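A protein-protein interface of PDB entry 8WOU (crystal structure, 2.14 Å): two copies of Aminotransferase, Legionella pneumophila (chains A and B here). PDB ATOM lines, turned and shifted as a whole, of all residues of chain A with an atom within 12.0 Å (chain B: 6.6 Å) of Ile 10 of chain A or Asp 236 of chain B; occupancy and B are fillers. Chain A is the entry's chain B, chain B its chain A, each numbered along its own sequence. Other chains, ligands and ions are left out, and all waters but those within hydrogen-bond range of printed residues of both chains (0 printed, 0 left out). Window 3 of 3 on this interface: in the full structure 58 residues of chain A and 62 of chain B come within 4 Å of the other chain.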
ATOM      1  N   MET A   8       4.619  10.111  10.368  1.00  0.00           N
ATOM      2  CA  MET A   8       5.834  10.827  10.741  1.00  0.00           C
ATOM      3  C   MET A   8       7.094  10.010  10.439  1.00  0.00           C
ATOM      4  O   MET A   8       8.158  10.580  10.184  1.00  0.00           O
ATOM      5  CB  MET A   8       5.797  11.200  12.226  1.00  0.00           C
ATOM      6  CG  MET A   8       7.014  11.987  12.713  1.00  0.00           C
ATOM      7  SD  MET A   8       7.049  12.262  14.503  1.00  0.00           S
ATOM      8  CE  MET A   8       8.310  11.092  15.004  1.00  0.00           C
ATOM      9  N   ASP A   9       6.976   8.682  10.456  1.00  0.00           N
ATOM     10  CA  ASP A   9       8.131   7.797  10.348  1.00  0.00           C
ATOM     11  C   ASP A   9       8.175   7.072   9.007  1.00  0.00           C
ATOM     12  O   ASP A   9       7.146   6.636   8.475  1.00  0.00           O
ATOM     13  CB  ASP A   9       8.151   6.766  11.479  1.00  0.00           C
ATOM     14  CG  ASP A   9       9.537   6.176  11.702  1.00  0.00           C
ATOM     15  OD1 ASP A   9      10.270   5.955  10.709  1.00  0.00           O
ATOM     16  OD2 ASP A   9       9.899   5.937  12.872  1.00  0.00           O
ATOM     17  N   ILE A  10       9.391   6.919   8.490  1.00  0.00           N
ATOM     18  CA  ILE A  10       9.623   6.264   7.209  1.00  0.00           C
ATOM     19  C   ILE A  10       9.476   4.760   7.391  1.00  0.00           C
ATOM     20  O   ILE A  10      10.131   4.162   8.252  1.00  0.00           O
ATOM     21  CB  ILE A  10      11.020   6.616   6.667  1.00  0.00           C
ATOM     22  CG1 ILE A  10      11.337   8.108   6.877  1.00  0.00           C
ATOM     23  CG2 ILE A  10      11.170   6.183   5.198  1.00  0.00           C
ATOM     24  CD1 ILE A  10      10.295   9.084   6.317  1.00  0.00           C
ATOM     25  N   ALA A  11       8.613   4.144   6.585  1.00  0.00           N
ATOM     26  CA  ALA A  11       8.487   2.693   6.551  1.00  0.00           C
ATOM     27  C   ALA A  11       9.537   2.106   5.613  1.00  0.00           C
ATOM     28  O   ALA A  11       9.785   2.640   4.529  1.00  0.00           O
ATOM     29  CB  ALA A  11       7.082   2.285   6.109  1.00  0.00           C
ATOM     30  N   LEU A  12      10.156   1.005   6.040  1.00  0.00           N
ATOM     31  CA  LEU A  12      11.325   0.428   5.386  1.00  0.00           C
ATOM     32  C   LEU A  12      10.984  -0.941   4.799  1.00  0.00           C
ATOM     33  O   LEU A  12       9.977  -1.557   5.158  1.00  0.00           O
ATOM     34  CB  LEU A  12      12.497   0.309   6.368  1.00  0.00           C
ATOM     35  CG  LEU A  12      13.356   1.543   6.689  1.00  0.00           C
ATOM     36  CD1 LEU A  12      12.558   2.829   6.796  1.00  0.00           C
ATOM     37  CD2 LEU A  12      14.079   1.293   7.978  1.00  0.00           C
ATOM     38  N   ALA A  13      11.838  -1.414   3.888  1.00  0.00           N
ATOM     39  CA  ALA A  13      11.478  -2.543   3.031  1.00  0.00           C
ATOM     40  C   ALA A  13      11.409  -3.846   3.814  1.00  0.00           C
ATOM     41  O   ALA A  13      12.230  -4.102   4.697  1.00  0.00           O
ATOM     42  CB  ALA A  13      12.482  -2.697   1.884  1.00  0.00           C
ATOM     43  N   LYS A  14      10.443  -4.697   3.458  1.00  0.00           N
ATOM     44  CA  LYS A  14      10.283  -5.960   4.176  1.00  0.00           C
ATOM     45  C   LYS A  14      11.562  -6.795   4.146  1.00  0.00           C
ATOM     46  O   LYS A  14      11.946  -7.388   5.160  1.00  0.00           O
ATOM     47  CB  LYS A  14       9.100  -6.738   3.603  1.00  0.00           C
ATOM     48  CG  LYS A  14       7.756  -6.095   3.976  1.00  0.00           C
ATOM     49  CD  LYS A  14       6.580  -6.894   3.425  1.00  0.00           C
ATOM     50  CE  LYS A  14       6.010  -6.272   2.149  1.00  0.00           C
ATOM     51  NZ  LYS A  14       4.919  -5.283   2.411  1.00  0.00           N
ATOM     52  N   VAL A  16      14.578  -5.881   4.262  1.00  0.00           N
ATOM     53  CA  VAL A  16      15.583  -5.489   5.237  1.00  0.00           C
ATOM     54  C   VAL A  16      15.171  -5.899   6.658  1.00  0.00           C
ATOM     55  O   VAL A  16      16.031  -6.026   7.538  1.00  0.00           O
ATOM     56  CB  VAL A  16      15.877  -3.983   5.132  1.00  0.00           C
ATOM     57  CG1 VAL A  16      14.821  -3.170   5.885  1.00  0.00           C
ATOM     58  CG2 VAL A  16      17.291  -3.682   5.617  1.00  0.00           C
ATOM     59  N   GLN A  17      13.880  -6.145   6.901  1.00  0.00           N
ATOM     60  CA  GLN A  17      13.445  -6.621   8.209  1.00  0.00           C
ATOM     61  C   GLN A  17      13.806  -8.079   8.453  1.00  0.00           C
ATOM     62  O   GLN A  17      13.740  -8.527   9.602  1.00  0.00           O
ATOM     63  CB  GLN A  17      11.933  -6.428   8.371  1.00  0.00           C
ATOM     64  CG  GLN A  17      11.510  -4.964   8.472  1.00  0.00           C
ATOM     65  CD  GLN A  17      10.124  -4.720   7.916  1.00  0.00           C
ATOM     66  OE1 GLN A  17       9.173  -5.410   8.274  1.00  0.00           O
ATOM     67  NE2 GLN A  17      10.005  -3.741   7.028  1.00  0.00           N
ATOM     68  N   TYR B 119      14.363   0.354   0.837  1.00  0.00           N
ATOM     69  CA  TYR B 119      13.100   1.061   1.023  1.00  0.00           C
ATOM     70  C   TYR B 119      11.932   0.477   0.247  1.00  0.00           C
ATOM     71  O   TYR B 119      10.794   0.557   0.725  1.00  0.00           O
ATOM     72  CB  TYR B 119      13.270   2.543   0.642  1.00  0.00           C
ATOM     73  CG  TYR B 119      11.996   3.369   0.693  1.00  0.00           C
ATOM     74  CD1 TYR B 119      11.497   3.848   1.901  1.00  0.00           C
ATOM     75  CD2 TYR B 119      11.301   3.667  -0.467  1.00  0.00           C
ATOM     76  CE1 TYR B 119      10.328   4.608   1.948  1.00  0.00           C
ATOM     77  CE2 TYR B 119      10.139   4.421  -0.430  1.00  0.00           C
ATOM     78  CZ  TYR B 119       9.660   4.889   0.768  1.00  0.00           C
ATOM     79  OH  TYR B 119       8.501   5.633   0.786  1.00  0.00           O
ATOM     80  N   ARG B 174       5.526   5.587  -3.968  1.00  0.00           N
ATOM     81  CA  ARG B 174       6.184   5.746  -2.677  1.00  0.00           C
ATOM     82  C   ARG B 174       7.535   6.439  -2.746  1.00  0.00           C
ATOM     83  O   ARG B 174       8.162   6.643  -1.699  1.00  0.00           O
ATOM     84  CB  ARG B 174       6.330   4.386  -1.983  1.00  0.00           C
ATOM     85  CG  ARG B 174       4.982   3.839  -1.502  1.00  0.00           C
ATOM     86  CD  ARG B 174       5.058   3.203  -0.116  1.00  0.00           C
ATOM     87  NE  ARG B 174       6.263   2.389   0.025  1.00  0.00           N
ATOM     88  CZ  ARG B 174       7.083   2.436   1.071  1.00  0.00           C
ATOM     89  NH1 ARG B 174       6.827   3.256   2.078  1.00  0.00           N
ATOM     90  NH2 ARG B 174       8.163   1.666   1.106  1.00  0.00           N
ATOM     91  N   PRO B 205       1.880  12.685   1.715  1.00  0.00           N
ATOM     92  CA  PRO B 205       2.949  12.509   2.713  1.00  0.00           C
ATOM     93  C   PRO B 205       3.638  11.152   2.677  1.00  0.00           C
ATOM     94  O   PRO B 205       4.675  10.996   3.334  1.00  0.00           O
ATOM     95  CB  PRO B 205       2.221  12.721   4.048  1.00  0.00           C
ATOM     96  CG  PRO B 205       0.809  12.346   3.757  1.00  0.00           C
ATOM     97  CD  PRO B 205       0.550  12.788   2.336  1.00  0.00           C
ATOM     98  N   LEU B 208       8.501   9.354  -0.588  1.00  0.00           N
ATOM     99  CA  LEU B 208       9.868   9.718  -0.252  1.00  0.00           C
ATOM    100  C   LEU B 208      10.534  10.394  -1.450  1.00  0.00           C
ATOM    101  O   LEU B 208      10.337   9.987  -2.596  1.00  0.00           O
ATOM    102  CB  LEU B 208      10.656   8.473   0.166  1.00  0.00           C
ATOM    103  CG  LEU B 208      12.162   8.673   0.363  1.00  0.00           C
ATOM    104  CD1 LEU B 208      12.442   9.378   1.692  1.00  0.00           C
ATOM    105  CD2 LEU B 208      12.961   7.359   0.241  1.00  0.00           C
ATOM    106  N   LEU B 228      15.023  20.863  -1.251  1.00  0.00           N
ATOM    107  CA  LEU B 228      14.902  21.178   0.165  1.00  0.00           C
ATOM    108  C   LEU B 228      15.114  22.661   0.440  1.00  0.00           C
ATOM    109  O   LEU B 228      14.499  23.201   1.358  1.00  0.00           O
ATOM    110  CB  LEU B 228      15.877  20.327   0.977  1.00  0.00           C
ATOM    111  CG  LEU B 228      15.353  18.903   1.118  1.00  0.00           C
ATOM    112  CD1 LEU B 228      16.163  18.075   2.110  1.00  0.00           C
ATOM    113  CD2 LEU B 228      13.876  18.936   1.507  1.00  0.00           C
ATOM    114  N   PRO B 232      11.589  23.649   2.527  1.00  0.00           N
ATOM    115  CA  PRO B 232      12.176  23.005   3.722  1.00  0.00           C
ATOM    116  C   PRO B 232      11.238  22.021   4.411  1.00  0.00           C
ATOM    117  O   PRO B 232      11.704  21.047   5.019  1.00  0.00           O
ATOM    118  CB  PRO B 232      12.497  24.198   4.637  1.00  0.00           C
ATOM    119  CG  PRO B 232      12.533  25.390   3.730  1.00  0.00           C
ATOM    120  CD  PRO B 232      11.551  25.120   2.636  1.00  0.00           C
ATOM    121  N   GLU B 233       9.924  22.249   4.323  1.00  0.00           N
ATOM    122  CA  GLU B 233       8.928  21.383   4.956  1.00  0.00           C
ATOM    123  C   GLU B 233       9.110  19.899   4.631  1.00  0.00           C
ATOM    124  O   GLU B 233       8.655  19.041   5.394  1.00  0.00           O
ATOM    125  CB  GLU B 233       7.523  21.824   4.528  1.00  0.00           C
ATOM    126  CG  GLU B 233       7.152  23.280   4.845  1.00  0.00           C
ATOM    127  CD  GLU B 233       7.811  24.301   3.914  1.00  0.00           C
ATOM    128  OE1 GLU B 233       8.189  25.388   4.405  1.00  0.00           O
ATOM    129  OE2 GLU B 233       7.959  24.021   2.704  1.00  0.00           O
ATOM    130  N   LEU B 234       9.731  19.570   3.497  1.00  0.00           N
ATOM    131  CA  LEU B 234       9.866  18.182   3.074  1.00  0.00           C
ATOM    132  C   LEU B 234      11.074  17.487   3.679  1.00  0.00           C
ATOM    133  O   LEU B 234      11.350  16.343   3.309  1.00  0.00           O
ATOM    134  CB  LEU B 234       9.964  18.090   1.552  1.00  0.00           C
ATOM    135  CG  LEU B 234       8.780  18.662   0.778  1.00  0.00           C
ATOM    136  CD1 LEU B 234       9.089  18.730  -0.721  1.00  0.00           C
ATOM    137  CD2 LEU B 234       7.538  17.834   1.060  1.00  0.00           C
ATOM    138  N   TYR B 235      11.796  18.153   4.579  1.00  0.00           N
ATOM    139  CA  TYR B 235      13.086  17.656   5.038  1.00  0.00           C
ATOM    140  C   TYR B 235      12.976  16.245   5.609  1.00  0.00           C
ATOM    141  O   TYR B 235      13.834  15.395   5.348  1.00  0.00           O
ATOM    142  CB  TYR B 235      13.645  18.622   6.089  1.00  0.00           C
ATOM    143  CG  TYR B 235      14.787  18.055   6.901  1.00  0.00           C
ATOM    144  CD1 TYR B 235      14.548  17.353   8.072  1.00  0.00           C
ATOM    145  CD2 TYR B 235      16.106  18.213   6.484  1.00  0.00           C
ATOM    146  CE1 TYR B 235      15.586  16.836   8.810  1.00  0.00           C
ATOM    147  CE2 TYR B 235      17.152  17.710   7.224  1.00  0.00           C
ATOM    148  CZ  TYR B 235      16.886  17.020   8.391  1.00  0.00           C
ATOM    149  OH  TYR B 235      17.926  16.509   9.149  1.00  0.00           O
ATOM    150  N   ASP B 236      11.937  15.983   6.413  1.00  0.00           N
ATOM    151  CA  ASP B 236      11.827  14.725   7.145  1.00  0.00           C
ATOM    152  C   ASP B 236      11.509  13.542   6.249  1.00  0.00           C
ATOM    153  O   ASP B 236      11.395  12.414   6.748  1.00  0.00           O
ATOM    154  CB  ASP B 236      10.762  14.844   8.240  1.00  0.00           C
ATOM    155  CG  ASP B 236       9.388  15.119   7.677  1.00  0.00           C
ATOM    156  OD1 ASP B 236       8.702  14.150   7.283  1.00  0.00           O
ATOM    157  OD2 ASP B 236       8.992  16.305   7.626  1.00  0.00           O
ATOM    158  N   ARG B 237      11.351  13.757   4.946  1.00  0.00           N
ATOM    159  CA  ARG B 237      11.080  12.661   4.029  1.00  0.00           C
ATOM    160  C   ARG B 237      11.838  12.860   2.726  1.00  0.00           C
ATOM    161  O   ARG B 237      11.333  12.565   1.641  1.00  0.00           O
ATOM    162  CB  ARG B 237       9.585  12.515   3.770  1.00  0.00           C
ATOM    163  CG  ARG B 237       8.910  13.783   3.285  1.00  0.00           C
ATOM    164  CD  ARG B 237       7.823  13.403   2.326  1.00  0.00           C
ATOM    165  NE  ARG B 237       6.638  14.244   2.414  1.00  0.00           N
ATOM    166  CZ  ARG B 237       5.752  14.347   1.431  1.00  0.00           C
ATOM    167  NH1 ARG B 237       5.944  13.652   0.310  1.00  0.00           N
ATOM    168  NH2 ARG B 237       4.671  15.119   1.564  1.00  0.00           N
ATOM    169  N   THR B 238      13.070  13.344   2.827  1.00  0.00           N
ATOM    170  CA  THR B 238      13.961  13.478   1.687  1.00  0.00           C
ATOM    171  C   THR B 238      15.303  12.838   2.002  1.00  0.00           C
ATOM    172  O   THR B 238      15.902  13.138   3.036  1.00  0.00           O
ATOM    173  CB  THR B 238      14.180  14.940   1.339  1.00  0.00           C
ATOM    174  OG1 THR B 238      12.921  15.557   1.033  1.00  0.00           O
ATOM    175  CG2 THR B 238      15.121  15.054   0.155  1.00  0.00           C
ATOM    176  N   PRO B 261      16.663  10.675   6.561  1.00  0.00           N
ATOM    177  CA  PRO B 261      16.128  10.251   7.853  1.00  0.00           C
ATOM    178  C   PRO B 261      16.944   9.099   8.424  1.00  0.00           C
ATOM    179  O   PRO B 261      17.315   8.162   7.713  1.00  0.00           O
ATOM    180  CB  PRO B 261      14.693   9.833   7.521  1.00  0.00           C
ATOM    181  CG  PRO B 261      14.369  10.596   6.246  1.00  0.00           C
ATOM    182  CD  PRO B 261      15.664  10.613   5.486  1.00  0.00           C
ATOM    183  N   PRO B 263      16.268   6.423  10.323  1.00  0.00           N
ATOM    184  CA  PRO B 263      15.871   5.019  10.130  1.00  0.00           C
ATOM    185  C   PRO B 263      16.157   4.513   8.728  1.00  0.00           C
ATOM    186  O   PRO B 263      16.527   3.346   8.561  1.00  0.00           O
ATOM    187  CB  PRO B 263      14.364   5.029  10.430  1.00  0.00           C
ATOM    188  CG  PRO B 263      14.144   6.245  11.265  1.00  0.00           C
ATOM    189  CD  PRO B 263      15.129   7.249  10.779  1.00  0.00           C
ATOM    190  N   LEU B 264      15.996   5.366   7.713  1.00  0.00           N
ATOM    191  CA  LEU B 264      16.291   4.948   6.345  1.00  0.00           C
ATOM    192  C   LEU B 264      17.788   4.776   6.140  1.00  0.00           C
ATOM    193  O   LEU B 264      18.227   3.841   5.462  1.00  0.00           O
ATOM    194  CB  LEU B 264      15.740   5.962   5.344  1.00  0.00           C
ATOM    195  CG  LEU B 264      16.111   5.616   3.896  1.00  0.00           C
ATOM    196  CD1 LEU B 264      15.436   4.324   3.486  1.00  0.00           C
ATOM    197  CD2 LEU B 264      15.735   6.720   2.919  1.00  0.00           C
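Among the printed residues, pairs that only touch across the chains: Leu 12 of chain A with Pro 263 of chain B (3.2 Å), Ala 11 of chain A with Tyr 119 of chain B (3.3 Å), Ile 10 of chain A with Asp 236 of chain B (3.5 Å), Ala 13 of chain A with Tyr 119 of chain B (3.6 Å), Ile 10 of chain A with Tyr 119 of chain B (3.7 Å), Ile 10 of chain A with Pro 261 of chain B (3.8 Å), Ala 11 of chain A with Arg 174 of chain B (3.9 Å) and Asp 9 of chain A with Pro 263 of chain B (3.9 Å).
O of Arg 174 of chain B lies within hydrogen-bond range of OH of Tyr 119 of chain B (2.7 Å).
The backbone NH (N) of Leu 208 of chain B lies within hydrogen-bond range of the backbone carbonyl oxygen (O) of Arg 174 of chain B.
NE2 of Gln 17 of chain A is in hydrogen-bond range of O of Leu 12 of chain A (2.9 Å).
The backbone carbonyl oxygen of Ala 13 of chain A sits at hydrogen-bond distance from the side-chain amide nitrogen of Gln 17 of chain A (3.2 Å).
No position is printed for both chains.
Of the 15 printed residues of chain B, 5 touch a printed residue of chain A.
Printed residues of chain B that touch a printed residue of chain A: Tyr 119, Arg 174, Asp 236, Pro 261 and Pro 263.
Hydrophobic or aromatic side chains of chain B that line the printed part of chain A: Tyr 119, Pro 261 and Pro 263.
Along chain B the printed residues that touch a printed residue of chain A span positions 119 to 263.
Printed residues of chain A that touch a printed residue of chain B: Asp 9, Ile 10, Ala 11, Leu 12 and Ala 13.
Hydrophobic or aromatic side chains of chain A that line the printed part of chain B: Ile 10, Leu 12 and Ala 13.
Among the printed residues, 8 pairs touch across the chains.
Of chain B, only Tyr 119, Asp 236 and Pro 261 come within 4 Å of Ile 10 of chain A.
Of the printed residues of chain B, Ala 11 of chain A touches Tyr 119 and Arg 174.
Of the printed residues of chain B, Leu 12 of chain A touches Pro 263.
Printed residues of chain B within 4 Å of Ala 13 of chain A: Tyr 119.
Tyr 119 of chain B touches three residues of chain A.
Tyr 235 of chain B touches none of the printed residues of chain A.
Of chain A, only Ile 10 comes within 4 Å of Asp 236 of chain B.
No residue of chain A comes within 4 Å of Thr 238 of chain B.
Pro 261 of chain B touches one residue of chain A.
The nearest residue of chain A that does not touch Asp 236 of chain B is Met 8 of chain A (4.6 Å).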
